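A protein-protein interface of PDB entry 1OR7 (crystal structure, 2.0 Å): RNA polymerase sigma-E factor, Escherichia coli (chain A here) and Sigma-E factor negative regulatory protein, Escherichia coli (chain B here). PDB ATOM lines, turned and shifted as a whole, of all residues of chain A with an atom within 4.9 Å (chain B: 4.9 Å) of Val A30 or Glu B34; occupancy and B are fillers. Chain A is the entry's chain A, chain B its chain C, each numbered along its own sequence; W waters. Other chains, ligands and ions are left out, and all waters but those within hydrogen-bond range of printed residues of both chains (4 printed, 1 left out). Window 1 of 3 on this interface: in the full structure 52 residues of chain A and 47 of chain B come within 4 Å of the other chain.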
ATOM      1  N   ASN A  26     -17.543  16.978 -18.266  1.00  0.00           N
ATOM      2  CA  ASN A  26     -17.718  18.134 -17.432  1.00  0.00           C
ATOM      3  C   ASN A  26     -16.563  18.263 -16.428  1.00  0.00           C
ATOM      4  O   ASN A  26     -16.070  19.367 -16.189  1.00  0.00           O
ATOM      5  CB  ASN A  26     -19.049  18.085 -16.684  1.00  0.00           C
ATOM      6  CG  ASN A  26     -19.159  19.197 -15.646  1.00  0.00           C
ATOM      7  OD1 ASN A  26     -18.990  20.372 -15.972  1.00  0.00           O
ATOM      8  ND2 ASN A  26     -19.385  18.817 -14.373  1.00  0.00           N
ATOM      9  N   LEU A  27     -16.147  17.141 -15.831  1.00  0.00           N
ATOM     10  CA  LEU A  27     -15.052  17.183 -14.865  1.00  0.00           C
ATOM     11  C   LEU A  27     -13.776  17.676 -15.528  1.00  0.00           C
ATOM     12  O   LEU A  27     -13.031  18.484 -14.920  1.00  0.00           O
ATOM     13  CB  LEU A  27     -14.803  15.832 -14.205  1.00  0.00           C
ATOM     14  CG  LEU A  27     -15.918  15.362 -13.295  1.00  0.00           C
ATOM     15  CD1 LEU A  27     -15.563  13.948 -12.789  1.00  0.00           C
ATOM     16  CD2 LEU A  27     -16.177  16.325 -12.140  1.00  0.00           C
ATOM     17  N   LEU A  28     -13.538  17.229 -16.762  1.00  0.00           N
ATOM     18  CA  LEU A  28     -12.338  17.623 -17.507  1.00  0.00           C
ATOM     19  C   LEU A  28     -12.382  19.084 -17.871  1.00  0.00           C
ATOM     20  O   LEU A  28     -11.370  19.755 -17.897  1.00  0.00           O
ATOM     21  CB  LEU A  28     -12.197  16.842 -18.836  1.00  0.00           C
ATOM     22  CG  LEU A  28     -11.610  15.470 -18.781  1.00  0.00           C
ATOM     23  CD1 LEU A  28     -11.777  14.808 -20.118  1.00  0.00           C
ATOM     24  CD2 LEU A  28     -10.150  15.516 -18.386  1.00  0.00           C
ATOM     25  N   VAL A  29     -13.563  19.569 -18.192  1.00  0.00           N
ATOM     26  CA  VAL A  29     -13.697  20.948 -18.611  1.00  0.00           C
ATOM     27  C   VAL A  29     -13.435  21.870 -17.419  1.00  0.00           C
ATOM     28  O   VAL A  29     -12.738  22.884 -17.555  1.00  0.00           O
ATOM     29  CB  VAL A  29     -15.077  21.207 -19.204  1.00  0.00           C
ATOM     30  CG1 VAL A  29     -15.237  22.667 -19.465  1.00  0.00           C
ATOM     31  CG2 VAL A  29     -15.245  20.423 -20.494  1.00  0.00           C
ATOM     32  N   VAL A  30     -13.979  21.498 -16.259  1.00  0.00           N
ATOM     33  CA  VAL A  30     -13.768  22.257 -15.018  1.00  0.00           C
ATOM     34  C   VAL A  30     -12.278  22.278 -14.699  1.00  0.00           C
ATOM     35  O   VAL A  30     -11.695  23.300 -14.290  1.00  0.00           O
ATOM     36  CB  VAL A  30     -14.579  21.672 -13.853  1.00  0.00           C
ATOM     37  CG1 VAL A  30     -14.198  22.271 -12.516  1.00  0.00           C
ATOM     38  CG2 VAL A  30     -16.080  21.889 -14.090  1.00  0.00           C
ATOM     39  N   ARG A  31     -11.640  21.143 -14.927  1.00  0.00           N
ATOM     40  CA  ARG A  31     -10.224  21.058 -14.672  1.00  0.00           C
ATOM     41  C   ARG A  31      -9.415  21.962 -15.596  1.00  0.00           C
ATOM     42  O   ARG A  31      -8.465  22.615 -15.158  1.00  0.00           O
ATOM     43  CB  ARG A  31      -9.814  19.633 -14.896  1.00  0.00           C
ATOM     44  CG  ARG A  31      -8.360  19.354 -14.878  1.00  0.00           C
ATOM     45  CD  ARG A  31      -8.101  18.470 -13.725  1.00  0.00           C
ATOM     46  NE  ARG A  31      -7.309  17.368 -14.080  1.00  0.00           N
ATOM     47  CZ  ARG A  31      -6.732  16.590 -13.217  1.00  0.00           C
ATOM     48  NH1 ARG A  31      -6.907  16.747 -11.902  1.00  0.00           N
ATOM     49  NH2 ARG A  31      -5.990  15.626 -13.677  1.00  0.00           N
ATOM     50  N   TYR A  32      -9.783  22.006 -16.869  1.00  0.00           N
ATOM     51  CA  TYR A  32      -8.986  22.708 -17.868  1.00  0.00           C
ATOM     52  C   TYR A  32      -9.494  24.105 -18.293  1.00  0.00           C
ATOM     53  O   TYR A  32      -8.831  24.792 -19.059  1.00  0.00           O
ATOM     54  CB  TYR A  32      -8.794  21.802 -19.127  1.00  0.00           C
ATOM     55  CG  TYR A  32      -7.790  20.758 -18.875  1.00  0.00           C
ATOM     56  CD1 TYR A  32      -8.160  19.471 -18.499  1.00  0.00           C
ATOM     57  CD2 TYR A  32      -6.447  21.068 -18.915  1.00  0.00           C
ATOM     58  CE1 TYR A  32      -7.188  18.502 -18.200  1.00  0.00           C
ATOM     59  CE2 TYR A  32      -5.515  20.147 -18.638  1.00  0.00           C
ATOM     60  CZ  TYR A  32      -5.874  18.871 -18.279  1.00  0.00           C
ATOM     61  OH  TYR A  32      -4.857  18.011 -17.968  1.00  0.00           O
ATOM     62  N   GLN A  33     -10.627  24.542 -17.776  1.00  0.00           N
ATOM     63  CA  GLN A  33     -11.231  25.809 -18.241  1.00  0.00           C
ATOM     64  C   GLN A  33     -10.367  27.066 -18.144  1.00  0.00           C
ATOM     65  O   GLN A  33     -10.319  27.808 -19.122  1.00  0.00           O
ATOM     66  CB  GLN A  33     -12.574  26.060 -17.547  1.00  0.00           C
ATOM     67  CG  GLN A  33     -12.488  26.200 -16.008  1.00  0.00           C
ATOM     68  CD  GLN A  33     -13.868  26.289 -15.349  1.00  0.00           C
ATOM     69  OE1 GLN A  33     -14.801  26.761 -15.972  1.00  0.00           O
ATOM     70  NE2 GLN A  33     -13.981  25.880 -14.088  1.00  0.00           N
ATOM     71  N   GLN B  30     -18.788  18.358  -6.585  1.00  0.00           N
ATOM     72  CA  GLN B  30     -18.518  19.062  -7.831  1.00  0.00           C
ATOM     73  C   GLN B  30     -18.002  20.472  -7.547  1.00  0.00           C
ATOM     74  O   GLN B  30     -17.068  20.959  -8.204  1.00  0.00           O
ATOM     75  CB  GLN B  30     -19.746  19.076  -8.740  1.00  0.00           C
ATOM     76  CG  GLN B  30     -19.953  17.732  -9.496  1.00  0.00           C
ATOM     77  CD  GLN B  30     -21.396  17.522  -9.936  1.00  0.00           C
ATOM     78  OE1 GLN B  30     -22.013  18.426 -10.500  1.00  0.00           O
ATOM     79  NE2 GLN B  30     -21.941  16.340  -9.667  1.00  0.00           N
ATOM     80  N   LYS B  31     -18.589  21.106  -6.542  1.00  0.00           N
ATOM     81  CA  LYS B  31     -18.154  22.453  -6.155  1.00  0.00           C
ATOM     82  C   LYS B  31     -16.740  22.437  -5.634  1.00  0.00           C
ATOM     83  O   LYS B  31     -15.943  23.329  -5.922  1.00  0.00           O
ATOM     84  CB  LYS B  31     -19.094  23.040  -5.095  1.00  0.00           C
ATOM     85  CG  LYS B  31     -20.128  23.946  -5.684  1.00  0.00           C
ATOM     86  N   THR B  32     -16.420  21.413  -4.855  1.00  0.00           N
ATOM     87  CA  THR B  32     -15.076  21.275  -4.315  1.00  0.00           C
ATOM     88  C   THR B  32     -14.070  21.005  -5.428  1.00  0.00           C
ATOM     89  O   THR B  32     -12.980  21.597  -5.456  1.00  0.00           O
ATOM     90  CB  THR B  32     -15.090  20.158  -3.277  1.00  0.00           C
ATOM     91  OG1 THR B  32     -16.053  20.482  -2.253  1.00  0.00           O
ATOM     92  CG2 THR B  32     -13.784  20.062  -2.581  1.00  0.00           C
ATOM     93  N   TRP B  33     -14.416  20.118  -6.346  1.00  0.00           N
ATOM     94  CA  TRP B  33     -13.557  19.881  -7.495  1.00  0.00           C
ATOM     95  C   TRP B  33     -13.259  21.201  -8.189  1.00  0.00           C
ATOM     96  O   TRP B  33     -12.135  21.472  -8.567  1.00  0.00           O
ATOM     97  CB  TRP B  33     -14.265  18.933  -8.474  1.00  0.00           C
ATOM     98  CG  TRP B  33     -13.551  18.545  -9.762  1.00  0.00           C
ATOM     99  CD1 TRP B  33     -13.814  19.023 -11.007  1.00  0.00           C
ATOM    100  CD2 TRP B  33     -12.604  17.493  -9.945  1.00  0.00           C
ATOM    101  NE1 TRP B  33     -13.054  18.375 -11.945  1.00  0.00           N
ATOM    102  CE2 TRP B  33     -12.299  17.431 -11.318  1.00  0.00           C
ATOM    103  CE3 TRP B  33     -11.962  16.617  -9.089  1.00  0.00           C
ATOM    104  CZ2 TRP B  33     -11.396  16.551 -11.836  1.00  0.00           C
ATOM    105  CZ3 TRP B  33     -11.052  15.736  -9.612  1.00  0.00           C
ATOM    106  CH2 TRP B  33     -10.773  15.708 -10.969  1.00  0.00           C
ATOM    107  N   GLU B  34     -14.295  21.996  -8.412  1.00  0.00           N
ATOM    108  CA  GLU B  34     -14.142  23.286  -9.074  1.00  0.00           C
ATOM    109  C   GLU B  34     -13.263  24.213  -8.245  1.00  0.00           C
ATOM    110  O   GLU B  34     -12.302  24.798  -8.771  1.00  0.00           O
ATOM    111  CB  GLU B  34     -15.535  23.890  -9.310  1.00  0.00           C
ATOM    112  CG  GLU B  34     -15.576  25.303  -9.836  1.00  0.00           C
ATOM    113  CD  GLU B  34     -17.011  25.794 -10.017  1.00  0.00           C
ATOM    114  OE1 GLU B  34     -17.656  26.139  -9.028  1.00  0.00           O
ATOM    115  OE2 GLU B  34     -17.510  25.809 -11.158  1.00  0.00           O
ATOM    116  N   SER B  35     -13.569  24.339  -6.950  1.00  0.00           N
ATOM    117  CA  SER B  35     -12.792  25.241  -6.098  1.00  0.00           C
ATOM    118  C   SER B  35     -11.317  24.860  -6.002  1.00  0.00           C
ATOM    119  O   SER B  35     -10.455  25.714  -6.137  1.00  0.00           O
ATOM    120  CB  SER B  35     -13.377  25.308  -4.693  1.00  0.00           C
ATOM    121  OG  SER B  35     -14.558  26.006  -4.778  1.00  0.00           O
ATOM    122  N   TYR B  36     -11.040  23.582  -5.783  1.00  0.00           N
ATOM    123  CA  TYR B  36      -9.653  23.113  -5.646  1.00  0.00           C
ATOM    124  C   TYR B  36      -8.851  23.282  -6.942  1.00  0.00           C
ATOM    125  O   TYR B  36      -7.665  23.577  -6.896  1.00  0.00           O
ATOM    126  CB  TYR B  36      -9.574  21.642  -5.172  1.00  0.00           C
ATOM    127  CG  TYR B  36      -9.985  21.367  -3.729  1.00  0.00           C
ATOM    128  CD1 TYR B  36     -10.385  22.387  -2.865  1.00  0.00           C
ATOM    129  CD2 TYR B  36     -10.019  20.061  -3.237  1.00  0.00           C
ATOM    130  CE1 TYR B  36     -10.790  22.109  -1.545  1.00  0.00           C
ATOM    131  CE2 TYR B  36     -10.412  19.783  -1.916  1.00  0.00           C
ATOM    132  CZ  TYR B  36     -10.785  20.807  -1.091  1.00  0.00           C
ATOM    133  OH  TYR B  36     -11.155  20.510   0.200  1.00  0.00           O
ATOM    134  N   HIS B  37      -9.490  23.078  -8.084  1.00  0.00           N
ATOM    135  CA  HIS B  37      -8.830  23.298  -9.350  1.00  0.00           C
ATOM    136  C   HIS B  37      -8.598  24.824  -9.569  1.00  0.00           C
ATOM    137  O   HIS B  37      -7.543  25.198 -10.060  1.00  0.00           O
ATOM    138  CB  HIS B  37      -9.563  22.608 -10.503  1.00  0.00           C
ATOM    139  CG  HIS B  37      -9.305  21.129 -10.578  1.00  0.00           C
ATOM    140  ND1 HIS B  37     -10.087  20.200  -9.927  1.00  0.00           N
ATOM    141  CD2 HIS B  37      -8.357  20.419 -11.242  1.00  0.00           C
ATOM    142  CE1 HIS B  37      -9.618  18.986 -10.171  1.00  0.00           C
ATOM    143  NE2 HIS B  37      -8.573  19.090 -10.969  1.00  0.00           N
ATOM    144  N   LEU B  38      -9.497  25.690  -9.098  1.00  0.00           N
ATOM    145  CA  LEU B  38      -9.263  27.143  -9.200  1.00  0.00           C
ATOM    146  C   LEU B  38      -8.008  27.508  -8.383  1.00  0.00           C
ATOM    147  O   LEU B  38      -7.111  28.218  -8.868  1.00  0.00           O
ATOM    148  CB  LEU B  38     -10.473  27.945  -8.735  1.00  0.00           C
ATOM    149  CG  LEU B  38     -10.351  29.485  -8.747  1.00  0.00           C
ATOM    150  CD1 LEU B  38     -10.038  29.999 -10.128  1.00  0.00           C
ATOM    151  CD2 LEU B  38     -11.624  30.096  -8.255  1.00  0.00           C
ATOM    152  N   SER B  56     -17.459  26.382 -17.949  1.00  0.00           N
ATOM    153  CA  SER B  56     -17.872  24.996 -18.025  1.00  0.00           C
ATOM    154  C   SER B  56     -19.363  24.881 -18.255  1.00  0.00           C
ATOM    155  O   SER B  56     -19.809  24.003 -18.973  1.00  0.00           O
ATOM    156  CB  SER B  56     -17.422  24.213 -16.776  1.00  0.00           C
ATOM    157  OG  SER B  56     -18.007  24.739 -15.586  1.00  0.00           O
HETATM  158  O   HOH W   1     -12.272  25.638 -11.505  1.00  0.00           O
HETATM  159  O   HOH W   2     -20.874  20.564 -12.102  1.00  0.00           O
HETATM  160  O   HOH W   3     -15.893  27.927 -12.583  1.00  0.00           O
HETATM  161  O   HOH W   4     -20.022  22.653 -14.972  1.00  0.00           O
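Water W4 lies within hydrogen-bond range of the side-chain amide oxygen of Asn A26 and the side-chain hydroxyl of Ser B56.
Water W1 bridges the backbone carbonyl oxygen of Glu B34 and the side-chain amide nitrogen of Gln A33.
Water W2 lies within hydrogen-bond range of OE1 of Gln B30 (2.9 Å) and ND2 of Asn A26 (3.2 Å).
Water W3 bridges OE2 of Glu B34 (3.0 Å) and NE2 of Gln A33 (3.2 Å).
Of the 8 printed residues of chain A, 5 touch a printed residue of chain B.
Printed residues of chain A that touch a printed residue of chain B: Leu A27, Val A29, Val A30, Arg A31 and Gln A33.
Hydrophobic or aromatic side chains of chain A within 4 Å of the printed part of chain B: Leu A27, Val A29 and Val A30.
Of the 10 printed residues of chain B, 4 touch a printed residue of chain A.
Hydrophobic or aromatic side chains of chain B within 4 Å of the printed part of chain A: Trp B33 and His B37.
Among the printed residues, 7 pairs touch across the chains.
The backbone carbonyl oxygen (O) of Trp B33 lies within hydrogen-bond range of a ring nitrogen (ND1) of His B37 (2.8 Å).
The backbone carbonyl oxygen (O) of Val A30 sits at hydrogen-bond distance from the side-chain amide nitrogen (NE2) of Gln A33 (3.5 Å).
Val A30 touches just these residues of chain B: Trp B33 (3.6 Å), Glu B34 (3.6 Å) and Ser B56 (3.8 Å).
Glu B34 touches just one residue of chain A: Val A30 (3.6 Å).
Printed residues of chain A within 4 Å of Trp B33: Leu A27 and Val A30.
Of the printed residues of chain B, Leu A27 touches Trp B33.
Of the printed residues of chain B, Gln A33 touches Ser B56 (3.3 Å).
Tyr B36 touches none of the printed residues of chain A.
The nearest residue of chain B that does not touch Val A30 is His B37 (4.4 Å).
The nearest residue of chain A that does not touch Glu B34 is Gln A33 (4.6 Å).
The nearest printed residue of chain B that does not touch Leu A27 is Gln B30 (4.8 Å).
Among the printed residues, merely in contact across the chains: Val A29 with Ser B56 (3.8 Å), Val A30 with Trp B33 (3.6 Å), Val A30 with Glu B34 (3.6 Å) and Val A30 with Ser B56 (3.8 Å).
The backbone carbonyl oxygen of Leu A27 is in hydrogen-bond range of the indole nitrogen of Trp B33, 3.0 Å away.
OE1 of Gln A33 is in hydrogen-bond range of N of Ser B56 (3.3 Å).
A ring nitrogen (NE2) of His B37 sits close to the guanidinium group of Arg A31, 3.0 Å away.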
